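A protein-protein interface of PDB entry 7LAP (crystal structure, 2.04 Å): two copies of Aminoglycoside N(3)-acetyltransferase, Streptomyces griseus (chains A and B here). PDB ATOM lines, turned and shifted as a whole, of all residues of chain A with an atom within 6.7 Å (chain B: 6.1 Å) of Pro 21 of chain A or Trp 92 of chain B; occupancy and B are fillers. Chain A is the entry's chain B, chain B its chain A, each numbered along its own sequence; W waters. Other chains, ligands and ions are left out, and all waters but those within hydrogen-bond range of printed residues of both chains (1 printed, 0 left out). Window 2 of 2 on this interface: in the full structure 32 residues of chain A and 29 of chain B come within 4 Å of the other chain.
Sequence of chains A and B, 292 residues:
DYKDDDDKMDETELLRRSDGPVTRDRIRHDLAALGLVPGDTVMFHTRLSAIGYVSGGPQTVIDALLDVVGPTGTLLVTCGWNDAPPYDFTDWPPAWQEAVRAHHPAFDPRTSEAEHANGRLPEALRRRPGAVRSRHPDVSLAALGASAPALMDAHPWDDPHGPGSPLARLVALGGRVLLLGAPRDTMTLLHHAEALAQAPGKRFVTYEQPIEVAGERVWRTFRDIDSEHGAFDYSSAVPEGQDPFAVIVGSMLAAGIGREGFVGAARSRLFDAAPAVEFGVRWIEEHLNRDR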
ATOM      1  N   LYS A   8      -9.781 -21.022   0.567  1.00  0.00           N
ATOM      2  CA  LYS A   8      -8.451 -20.540   0.186  1.00  0.00           C
ATOM      3  C   LYS A   8      -7.550 -21.619  -0.425  1.00  0.00           C
ATOM      4  O   LYS A   8      -6.967 -21.421  -1.497  1.00  0.00           O
ATOM      5  CB  LYS A   8      -7.787 -19.944   1.442  1.00  0.00           C
ATOM      6  CG  LYS A   8      -6.700 -18.939   1.223  1.00  0.00           C
ATOM      7  CD  LYS A   8      -7.177 -17.824   0.323  1.00  0.00           C
ATOM      8  CE  LYS A   8      -6.001 -16.974  -0.065  1.00  0.00           C
ATOM      9  NZ  LYS A   8      -4.719 -17.750   0.062  1.00  0.00           N
ATOM     10  N   GLU A  11      -8.683 -23.140  -3.778  1.00  0.00           N
ATOM     11  CA  GLU A  11      -8.398 -22.193  -4.851  1.00  0.00           C
ATOM     12  C   GLU A  11      -6.914 -22.176  -5.197  1.00  0.00           C
ATOM     13  O   GLU A  11      -6.561 -22.180  -6.375  1.00  0.00           O
ATOM     14  CB  GLU A  11      -8.878 -20.792  -4.481  1.00  0.00           C
ATOM     15  CG  GLU A  11     -10.392 -20.609  -4.631  1.00  0.00           C
ATOM     16  CD  GLU A  11     -10.913 -19.395  -3.884  1.00  0.00           C
ATOM     17  OE1 GLU A  11     -10.089 -18.651  -3.286  1.00  0.00           O
ATOM     18  OE2 GLU A  11     -12.150 -19.211  -3.864  1.00  0.00           O
ATOM     19  N   LEU A  14      -6.008 -25.318  -7.245  1.00  0.00           N
ATOM     20  CA  LEU A  14      -6.525 -25.307  -8.604  1.00  0.00           C
ATOM     21  C   LEU A  14      -5.789 -24.281  -9.470  1.00  0.00           C
ATOM     22  O   LEU A  14      -5.504 -24.552 -10.642  1.00  0.00           O
ATOM     23  CB  LEU A  14      -8.032 -25.047  -8.599  1.00  0.00           C
ATOM     24  CG  LEU A  14      -8.889 -26.163  -7.972  1.00  0.00           C
ATOM     25  CD1 LEU A  14     -10.361 -25.784  -7.915  1.00  0.00           C
ATOM     26  CD2 LEU A  14      -8.700 -27.454  -8.715  1.00  0.00           C
ATOM     27  N   LEU A  15      -5.506 -23.098  -8.919  1.00  0.00           N
ATOM     28  CA  LEU A  15      -4.725 -22.107  -9.664  1.00  0.00           C
ATOM     29  C   LEU A  15      -3.358 -22.671 -10.053  1.00  0.00           C
ATOM     30  O   LEU A  15      -2.933 -22.552 -11.203  1.00  0.00           O
ATOM     31  CB  LEU A  15      -4.563 -20.841  -8.828  1.00  0.00           C
ATOM     32  CG  LEU A  15      -5.819 -19.957  -8.710  1.00  0.00           C
ATOM     33  CD1 LEU A  15      -5.621 -18.935  -7.589  1.00  0.00           C
ATOM     34  CD2 LEU A  15      -6.140 -19.291 -10.044  1.00  0.00           C
ATOM     35  N   SER A  18      -3.620 -25.315 -13.087  1.00  0.00           N
ATOM     36  CA  SER A  18      -3.764 -24.779 -14.438  1.00  0.00           C
ATOM     37  C   SER A  18      -2.842 -23.594 -14.723  1.00  0.00           C
ATOM     38  O   SER A  18      -2.975 -22.966 -15.780  1.00  0.00           O
ATOM     39  CB  SER A  18      -5.219 -24.377 -14.695  1.00  0.00           C
ATOM     40  OG  SER A  18      -5.750 -23.607 -13.648  1.00  0.00           O
ATOM     41  N   ASP A  19      -1.930 -23.271 -13.811  1.00  0.00           N
ATOM     42  CA  ASP A  19      -1.066 -22.088 -13.934  1.00  0.00           C
ATOM     43  C   ASP A  19      -1.879 -20.812 -14.161  1.00  0.00           C
ATOM     44  O   ASP A  19      -1.563 -19.979 -15.012  1.00  0.00           O
ATOM     45  CB  ASP A  19      -0.036 -22.272 -15.045  1.00  0.00           C
ATOM     46  CG  ASP A  19       1.173 -21.379 -14.846  1.00  0.00           C
ATOM     47  OD1 ASP A  19       1.646 -21.239 -13.682  1.00  0.00           O
ATOM     48  OD2 ASP A  19       1.640 -20.815 -15.852  1.00  0.00           O
ATOM     49  N   GLY A  20      -2.932 -20.653 -13.376  1.00  0.00           N
ATOM     50  CA  GLY A  20      -3.716 -19.455 -13.423  1.00  0.00           C
ATOM     51  C   GLY A  20      -5.126 -19.778 -13.845  1.00  0.00           C
ATOM     52  O   GLY A  20      -5.435 -20.921 -14.211  1.00  0.00           O
ATOM     53  N   PRO A  21      -5.997 -18.763 -13.809  1.00  0.00           N
ATOM     54  CA  PRO A  21      -7.408 -18.958 -14.181  1.00  0.00           C
ATOM     55  C   PRO A  21      -7.581 -19.531 -15.580  1.00  0.00           C
ATOM     56  O   PRO A  21      -6.848 -19.200 -16.517  1.00  0.00           O
ATOM     57  CB  PRO A  21      -8.004 -17.541 -14.109  1.00  0.00           C
ATOM     58  CG  PRO A  21      -7.007 -16.728 -13.271  1.00  0.00           C
ATOM     59  CD  PRO A  21      -5.664 -17.352 -13.554  1.00  0.00           C
ATOM     60  N   VAL A  22      -8.586 -20.375 -15.719  1.00  0.00           N
ATOM     61  CA  VAL A  22      -8.972 -20.947 -17.005  1.00  0.00           C
ATOM     62  C   VAL A  22     -10.247 -20.237 -17.435  1.00  0.00           C
ATOM     63  O   VAL A  22     -11.238 -20.244 -16.695  1.00  0.00           O
ATOM     64  CB  VAL A  22      -9.187 -22.466 -16.900  1.00  0.00           C
ATOM     65  CG1 VAL A  22      -9.668 -23.000 -18.196  1.00  0.00           C
ATOM     66  CG2 VAL A  22      -7.849 -23.192 -16.461  1.00  0.00           C
ATOM     67  N   THR A  23     -10.217 -19.586 -18.594  1.00  0.00           N
ATOM     68  CA  THR A  23     -11.349 -18.760 -18.993  1.00  0.00           C
ATOM     69  C   THR A  23     -12.217 -19.442 -20.049  1.00  0.00           C
ATOM     70  O   THR A  23     -11.827 -20.420 -20.685  1.00  0.00           O
ATOM     71  CB  THR A  23     -10.855 -17.444 -19.549  1.00  0.00           C
ATOM     72  OG1 THR A  23     -10.174 -17.723 -20.788  1.00  0.00           O
ATOM     73  CG2 THR A  23      -9.929 -16.783 -18.540  1.00  0.00           C
ATOM     74  N   ARG A  26     -10.574 -19.719 -23.474  1.00  0.00           N
ATOM     75  CA  ARG A  26      -9.498 -20.692 -23.542  1.00  0.00           C
ATOM     76  C   ARG A  26     -10.047 -22.107 -23.620  1.00  0.00           C
ATOM     77  O   ARG A  26      -9.511 -22.954 -24.346  1.00  0.00           O
ATOM     78  CB  ARG A  26      -8.574 -20.539 -22.333  1.00  0.00           C
ATOM     79  CG  ARG A  26      -7.350 -21.431 -22.426  1.00  0.00           C
ATOM     80  CD  ARG A  26      -7.581 -22.641 -21.612  1.00  0.00           C
ATOM     81  NE  ARG A  26      -6.436 -23.547 -21.642  1.00  0.00           N
ATOM     82  CZ  ARG A  26      -5.360 -23.410 -20.876  1.00  0.00           C
ATOM     83  NH1 ARG A  26      -5.253 -22.381 -20.049  1.00  0.00           N
ATOM     84  NH2 ARG A  26      -4.404 -24.295 -20.954  1.00  0.00           N
ATOM     85  N   TYR A  53      -8.480 -24.047 -12.123  1.00  0.00           N
ATOM     86  CA  TYR A  53      -9.336 -22.999 -11.551  1.00  0.00           C
ATOM     87  C   TYR A  53     -10.141 -22.386 -12.688  1.00  0.00           C
ATOM     88  O   TYR A  53      -9.608 -21.633 -13.510  1.00  0.00           O
ATOM     89  CB  TYR A  53      -8.509 -21.940 -10.805  1.00  0.00           C
ATOM     90  CG  TYR A  53      -9.449 -20.868 -10.288  1.00  0.00           C
ATOM     91  CD1 TYR A  53     -10.178 -21.048  -9.117  1.00  0.00           C
ATOM     92  CD2 TYR A  53      -9.667 -19.705 -11.022  1.00  0.00           C
ATOM     93  CE1 TYR A  53     -11.100 -20.059  -8.675  1.00  0.00           C
ATOM     94  CE2 TYR A  53     -10.577 -18.739 -10.601  1.00  0.00           C
ATOM     95  CZ  TYR A  53     -11.292 -18.907  -9.436  1.00  0.00           C
ATOM     96  OH  TYR A  53     -12.209 -17.902  -9.073  1.00  0.00           O
ATOM     97  N   VAL A  54     -11.428 -22.721 -12.780  1.00  0.00           N
ATOM     98  CA  VAL A  54     -12.245 -22.248 -13.887  1.00  0.00           C
ATOM     99  C   VAL A  54     -12.971 -20.983 -13.433  1.00  0.00           C
ATOM    100  O   VAL A  54     -13.774 -21.021 -12.496  1.00  0.00           O
ATOM    101  CB  VAL A  54     -13.234 -23.316 -14.374  1.00  0.00           C
ATOM    102  CG1 VAL A  54     -14.197 -22.688 -15.433  1.00  0.00           C
ATOM    103  CG2 VAL A  54     -12.492 -24.490 -15.001  1.00  0.00           C
ATOM    104  N   SER A  55     -12.672 -19.865 -14.091  1.00  0.00           N
ATOM    105  CA  SER A  55     -13.215 -18.555 -13.727  1.00  0.00           C
ATOM    106  C   SER A  55     -14.703 -18.536 -14.054  1.00  0.00           C
ATOM    107  O   SER A  55     -15.090 -18.407 -15.222  1.00  0.00           O
ATOM    108  CB  SER A  55     -12.469 -17.458 -14.486  1.00  0.00           C
ATOM    109  OG  SER A  55     -13.045 -16.177 -14.281  1.00  0.00           O
ATOM    110  N   PRO B  86     -12.615 -14.538  -5.783  1.00  0.00           N
ATOM    111  CA  PRO B  86     -12.168 -14.365  -4.385  1.00  0.00           C
ATOM    112  C   PRO B  86     -11.885 -12.903  -4.070  1.00  0.00           C
ATOM    113  O   PRO B  86     -11.464 -12.137  -4.941  1.00  0.00           O
ATOM    114  CB  PRO B  86     -10.874 -15.192  -4.315  1.00  0.00           C
ATOM    115  CG  PRO B  86     -10.893 -16.064  -5.515  1.00  0.00           C
ATOM    116  CD  PRO B  86     -11.726 -15.385  -6.581  1.00  0.00           C
ATOM    117  N   ASP B  88      -9.574 -11.480  -2.687  1.00  0.00           N
ATOM    118  CA  ASP B  88      -8.183 -11.088  -2.844  1.00  0.00           C
ATOM    119  C   ASP B  88      -7.582 -11.465  -4.208  1.00  0.00           C
ATOM    120  O   ASP B  88      -6.355 -11.536  -4.324  1.00  0.00           O
ATOM    121  CB  ASP B  88      -7.349 -11.693  -1.720  1.00  0.00           C
ATOM    122  CG  ASP B  88      -7.310 -13.203  -1.787  1.00  0.00           C
ATOM    123  OD1 ASP B  88      -8.177 -13.799  -2.460  1.00  0.00           O
ATOM    124  OD2 ASP B  88      -6.405 -13.804  -1.186  1.00  0.00           O
ATOM    125  N   PHE B  89      -8.410 -11.695  -5.241  1.00  0.00           N
ATOM    126  CA  PHE B  89      -7.866 -11.916  -6.579  1.00  0.00           C
ATOM    127  C   PHE B  89      -7.017 -10.727  -7.037  1.00  0.00           C
ATOM    128  O   PHE B  89      -6.155 -10.889  -7.903  1.00  0.00           O
ATOM    129  CB  PHE B  89      -9.003 -12.231  -7.592  1.00  0.00           C
ATOM    130  CG  PHE B  89      -9.651 -11.018  -8.215  1.00  0.00           C
ATOM    131  CD1 PHE B  89     -10.745 -10.404  -7.612  1.00  0.00           C
ATOM    132  CD2 PHE B  89      -9.172 -10.507  -9.416  1.00  0.00           C
ATOM    133  CE1 PHE B  89     -11.369  -9.271  -8.185  1.00  0.00           C
ATOM    134  CE2 PHE B  89      -9.761  -9.369 -10.016  1.00  0.00           C
ATOM    135  CZ  PHE B  89     -10.860  -8.738  -9.384  1.00  0.00           C
ATOM    136  N   THR B  90      -7.206  -9.551  -6.449  1.00  0.00           N
ATOM    137  CA  THR B  90      -6.385  -8.405  -6.807  1.00  0.00           C
ATOM    138  C   THR B  90      -4.999  -8.471  -6.181  1.00  0.00           C
ATOM    139  O   THR B  90      -4.178  -7.591  -6.466  1.00  0.00           O
ATOM    140  CB  THR B  90      -7.085  -7.093  -6.407  1.00  0.00           C
ATOM    141  OG1 THR B  90      -7.648  -7.265  -5.118  1.00  0.00           O
ATOM    142  CG2 THR B  90      -8.196  -6.740  -7.393  1.00  0.00           C
ATOM    143  N   ASP B  91      -4.710  -9.502  -5.374  1.00  0.00           N
ATOM    144  CA  ASP B  91      -3.335  -9.828  -5.012  1.00  0.00           C
ATOM    145  C   ASP B  91      -2.657 -10.784  -5.992  1.00  0.00           C
ATOM    146  O   ASP B  91      -1.460 -11.011  -5.875  1.00  0.00           O
ATOM    147  CB  ASP B  91      -3.286 -10.463  -3.626  1.00  0.00           C
ATOM    148  CG  ASP B  91      -3.718  -9.511  -2.531  1.00  0.00           C
ATOM    149  OD1 ASP B  91      -3.752  -8.283  -2.756  1.00  0.00           O
ATOM    150  OD2 ASP B  91      -4.046 -10.010  -1.433  1.00  0.00           O
ATOM    151  N   TRP B  92      -3.380 -11.390  -6.923  1.00  0.00           N
ATOM    152  CA  TRP B  92      -2.778 -12.375  -7.818  1.00  0.00           C
ATOM    153  C   TRP B  92      -1.767 -11.728  -8.774  1.00  0.00           C
ATOM    154  O   TRP B  92      -1.761 -10.512  -8.963  1.00  0.00           O
ATOM    155  CB  TRP B  92      -3.881 -13.069  -8.633  1.00  0.00           C
ATOM    156  CG  TRP B  92      -4.806 -13.914  -7.804  1.00  0.00           C
ATOM    157  CD1 TRP B  92      -4.706 -14.180  -6.457  1.00  0.00           C
ATOM    158  CD2 TRP B  92      -5.985 -14.591  -8.262  1.00  0.00           C
ATOM    159  NE1 TRP B  92      -5.758 -14.992  -6.059  1.00  0.00           N
ATOM    160  CE2 TRP B  92      -6.544 -15.269  -7.149  1.00  0.00           C
ATOM    161  CE3 TRP B  92      -6.613 -14.708  -9.509  1.00  0.00           C
ATOM    162  CZ2 TRP B  92      -7.722 -16.014  -7.242  1.00  0.00           C
ATOM    163  CZ3 TRP B  92      -7.778 -15.465  -9.602  1.00  0.00           C
ATOM    164  CH2 TRP B  92      -8.325 -16.096  -8.472  1.00  0.00           C
ATOM    165  N   PRO B  93      -0.925 -12.528  -9.427  1.00  0.00           N
ATOM    166  CA  PRO B  93      -0.067 -11.990 -10.511  1.00  0.00           C
ATOM    167  C   PRO B  93      -0.889 -11.216 -11.535  1.00  0.00           C
ATOM    168  O   PRO B  93      -2.035 -11.580 -11.833  1.00  0.00           O
ATOM    169  CB  PRO B  93       0.559 -13.253 -11.135  1.00  0.00           C
ATOM    170  CG  PRO B  93       0.533 -14.280 -10.000  1.00  0.00           C
ATOM    171  CD  PRO B  93      -0.736 -13.977  -9.222  1.00  0.00           C
ATOM    172  N   PRO B  94      -0.322 -10.148 -12.111  1.00  0.00           N
ATOM    173  CA  PRO B  94      -1.113  -9.270 -12.997  1.00  0.00           C
ATOM    174  C   PRO B  94      -1.837  -9.990 -14.117  1.00  0.00           C
ATOM    175  O   PRO B  94      -2.973  -9.623 -14.430  1.00  0.00           O
ATOM    176  CB  PRO B  94      -0.065  -8.296 -13.555  1.00  0.00           C
ATOM    177  CG  PRO B  94       0.994  -8.228 -12.491  1.00  0.00           C
ATOM    178  CD  PRO B  94       1.049  -9.647 -11.892  1.00  0.00           C
ATOM    179  N   ALA B  95      -1.223 -11.009 -14.727  1.00  0.00           N
ATOM    180  CA  ALA B  95      -1.900 -11.711 -15.808  1.00  0.00           C
ATOM    181  C   ALA B  95      -3.119 -12.455 -15.302  1.00  0.00           C
ATOM    182  O   ALA B  95      -4.127 -12.563 -16.010  1.00  0.00           O
ATOM    183  CB  ALA B  95      -0.947 -12.693 -16.483  1.00  0.00           C
ATOM    184  N   TRP B  96      -3.033 -13.024 -14.098  1.00  0.00           N
ATOM    185  CA  TRP B  96      -4.178 -13.751 -13.575  1.00  0.00           C
ATOM    186  C   TRP B  96      -5.322 -12.797 -13.266  1.00  0.00           C
ATOM    187  O   TRP B  96      -6.467 -13.102 -13.574  1.00  0.00           O
ATOM    188  CB  TRP B  96      -3.803 -14.535 -12.313  1.00  0.00           C
ATOM    189  CG  TRP B  96      -2.761 -15.591 -12.522  1.00  0.00           C
ATOM    190  CD1 TRP B  96      -1.978 -15.786 -13.637  1.00  0.00           C
ATOM    191  CD2 TRP B  96      -2.361 -16.584 -11.571  1.00  0.00           C
ATOM    192  NE1 TRP B  96      -1.118 -16.840 -13.422  1.00  0.00           N
ATOM    193  CE2 TRP B  96      -1.333 -17.344 -12.165  1.00  0.00           C
ATOM    194  CE3 TRP B  96      -2.775 -16.899 -10.271  1.00  0.00           C
ATOM    195  CZ2 TRP B  96      -0.720 -18.407 -11.510  1.00  0.00           C
ATOM    196  CZ3 TRP B  96      -2.169 -17.952  -9.626  1.00  0.00           C
ATOM    197  CH2 TRP B  96      -1.148 -18.691 -10.245  1.00  0.00           C
ATOM    198  N   GLN B  97      -5.046 -11.640 -12.642  1.00  0.00           N
ATOM    199  CA  GLN B  97      -6.189 -10.797 -12.330  1.00  0.00           C
ATOM    200  C   GLN B  97      -6.766 -10.152 -13.576  1.00  0.00           C
ATOM    201  O   GLN B  97      -7.965  -9.896 -13.614  1.00  0.00           O
ATOM    202  CB  GLN B  97      -5.876  -9.739 -11.266  1.00  0.00           C
ATOM    203  CG  GLN B  97      -4.640  -9.008 -11.339  1.00  0.00           C
ATOM    204  CD  GLN B  97      -4.514  -8.035 -10.151  1.00  0.00           C
ATOM    205  OE1 GLN B  97      -5.322  -7.105 -10.012  1.00  0.00           O
ATOM    206  NE2 GLN B  97      -3.500  -8.250  -9.297  1.00  0.00           N
ATOM    207  N   ALA B  99      -7.116 -11.706 -16.406  1.00  0.00           N
ATOM    208  CA  ALA B  99      -8.018 -12.717 -16.938  1.00  0.00           C
ATOM    209  C   ALA B  99      -9.358 -12.728 -16.184  1.00  0.00           C
ATOM    210  O   ALA B  99     -10.433 -12.808 -16.806  1.00  0.00           O
ATOM    211  CB  ALA B  99      -7.336 -14.083 -16.876  1.00  0.00           C
ATOM    212  N   VAL B 100      -9.323 -12.646 -14.847  1.00  0.00           N
ATOM    213  CA  VAL B 100     -10.572 -12.522 -14.081  1.00  0.00           C
ATOM    214  C   VAL B 100     -11.330 -11.269 -14.504  1.00  0.00           C
ATOM    215  O   VAL B 100     -12.535 -11.315 -14.775  1.00  0.00           O
ATOM    216  CB  VAL B 100     -10.291 -12.514 -12.563  1.00  0.00           C
ATOM    217  CG1 VAL B 100     -11.582 -12.225 -11.767  1.00  0.00           C
ATOM    218  CG2 VAL B 100      -9.674 -13.840 -12.112  1.00  0.00           C
HETATM  219  O   HOH W   1       0.536 -17.998 -15.368  1.00  0.00           O
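Among the printed residues, pairs that only touch across the chains: Lys 8 of chain A with Asp 88 of chain B, Glu 11 of chain A with Pro 86 of chain B, Leu 15 of chain A with Trp 92 of chain B, Leu 15 of chain A with Trp 96 of chain B, Asp 19 of chain A with Trp 96 of chain B, Gly 20 of chain A with Trp 96 of chain B, Pro 21 of chain A with Trp 92 of chain B, Pro 21 of chain A with Trp 96 of chain B and Tyr 53 of chain A with Pro 86 of chain B.
The side-chain hydroxyl (OG) of Ser 18 of chain A is in hydrogen-bond range of the backbone NH (N) of Tyr 53 of chain A (3.2 Å).
O of Trp 92 of chain B sits at hydrogen-bond distance from NE2 of Gln 97 of chain B (2.9 Å).
The backbone carbonyl oxygen (O) of Gly 20 of chain A lies within hydrogen-bond range of the side-chain hydroxyl (OG) of Ser 18 of chain A (2.8 Å).
O of Leu 14 of chain A lies within hydrogen-bond range of N of Tyr 53 of chain A (3.4 Å).
N of Val 22 of chain A is in hydrogen-bond range of O of Tyr 53 of chain A.
O of Leu 15 of chain A is in hydrogen-bond range of N of Gly 20 of chain A (2.9 Å).
Water W1 bridges NE1 of Trp 96 of chain B (2.8 Å) and O of Asp 19 of chain A (2.9 Å).
Of chain A, only Leu 15 and Pro 21 come within 4 Å of Trp 92 of chain B.
Of the printed residues of chain B, Gly 20 of chain A touches Trp 96 (3.4 Å).
Printed residues of chain A within 4 Å of Trp 96 of chain B: Leu 15 (3.8 Å), Asp 19 (3.5 Å), Gly 20 (3.4 Å) and Pro 21 (3.5 Å).
Printed residues of chain B within 4 Å of Leu 15 of chain A: Trp 92 (3.6 Å) and Trp 96 (3.8 Å).
Val 22 of chain A touches none of the printed residues of chain B.
Gln 97 of chain B touches none of the printed residues of chain A.
The nearest residue of chain A that does not touch Trp 92 of chain B is Tyr 53 of chain A (4.1 Å).
No position is printed for both chains.
Printed residues of chain A that touch a printed residue of chain B: Lys 8, Glu 11, Leu 15, Asp 19, Gly 20, Pro 21 and Tyr 53.
Hydrophobic or aromatic side chains of chain A within 4 Å of the printed part of chain B: Leu 15, Pro 21 and Tyr 53.
Hydrophobic or aromatic side chains of chain B within 4 Å of the printed part of chain A: Pro 86, Trp 92 and Trp 96.
Among the printed residues, 9 pairs touch across the chains.
Among the printed residues, no Asp or Glu carboxylate lies within 4 Å of a Lys or Arg side-chain nitrogen of the other chain.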
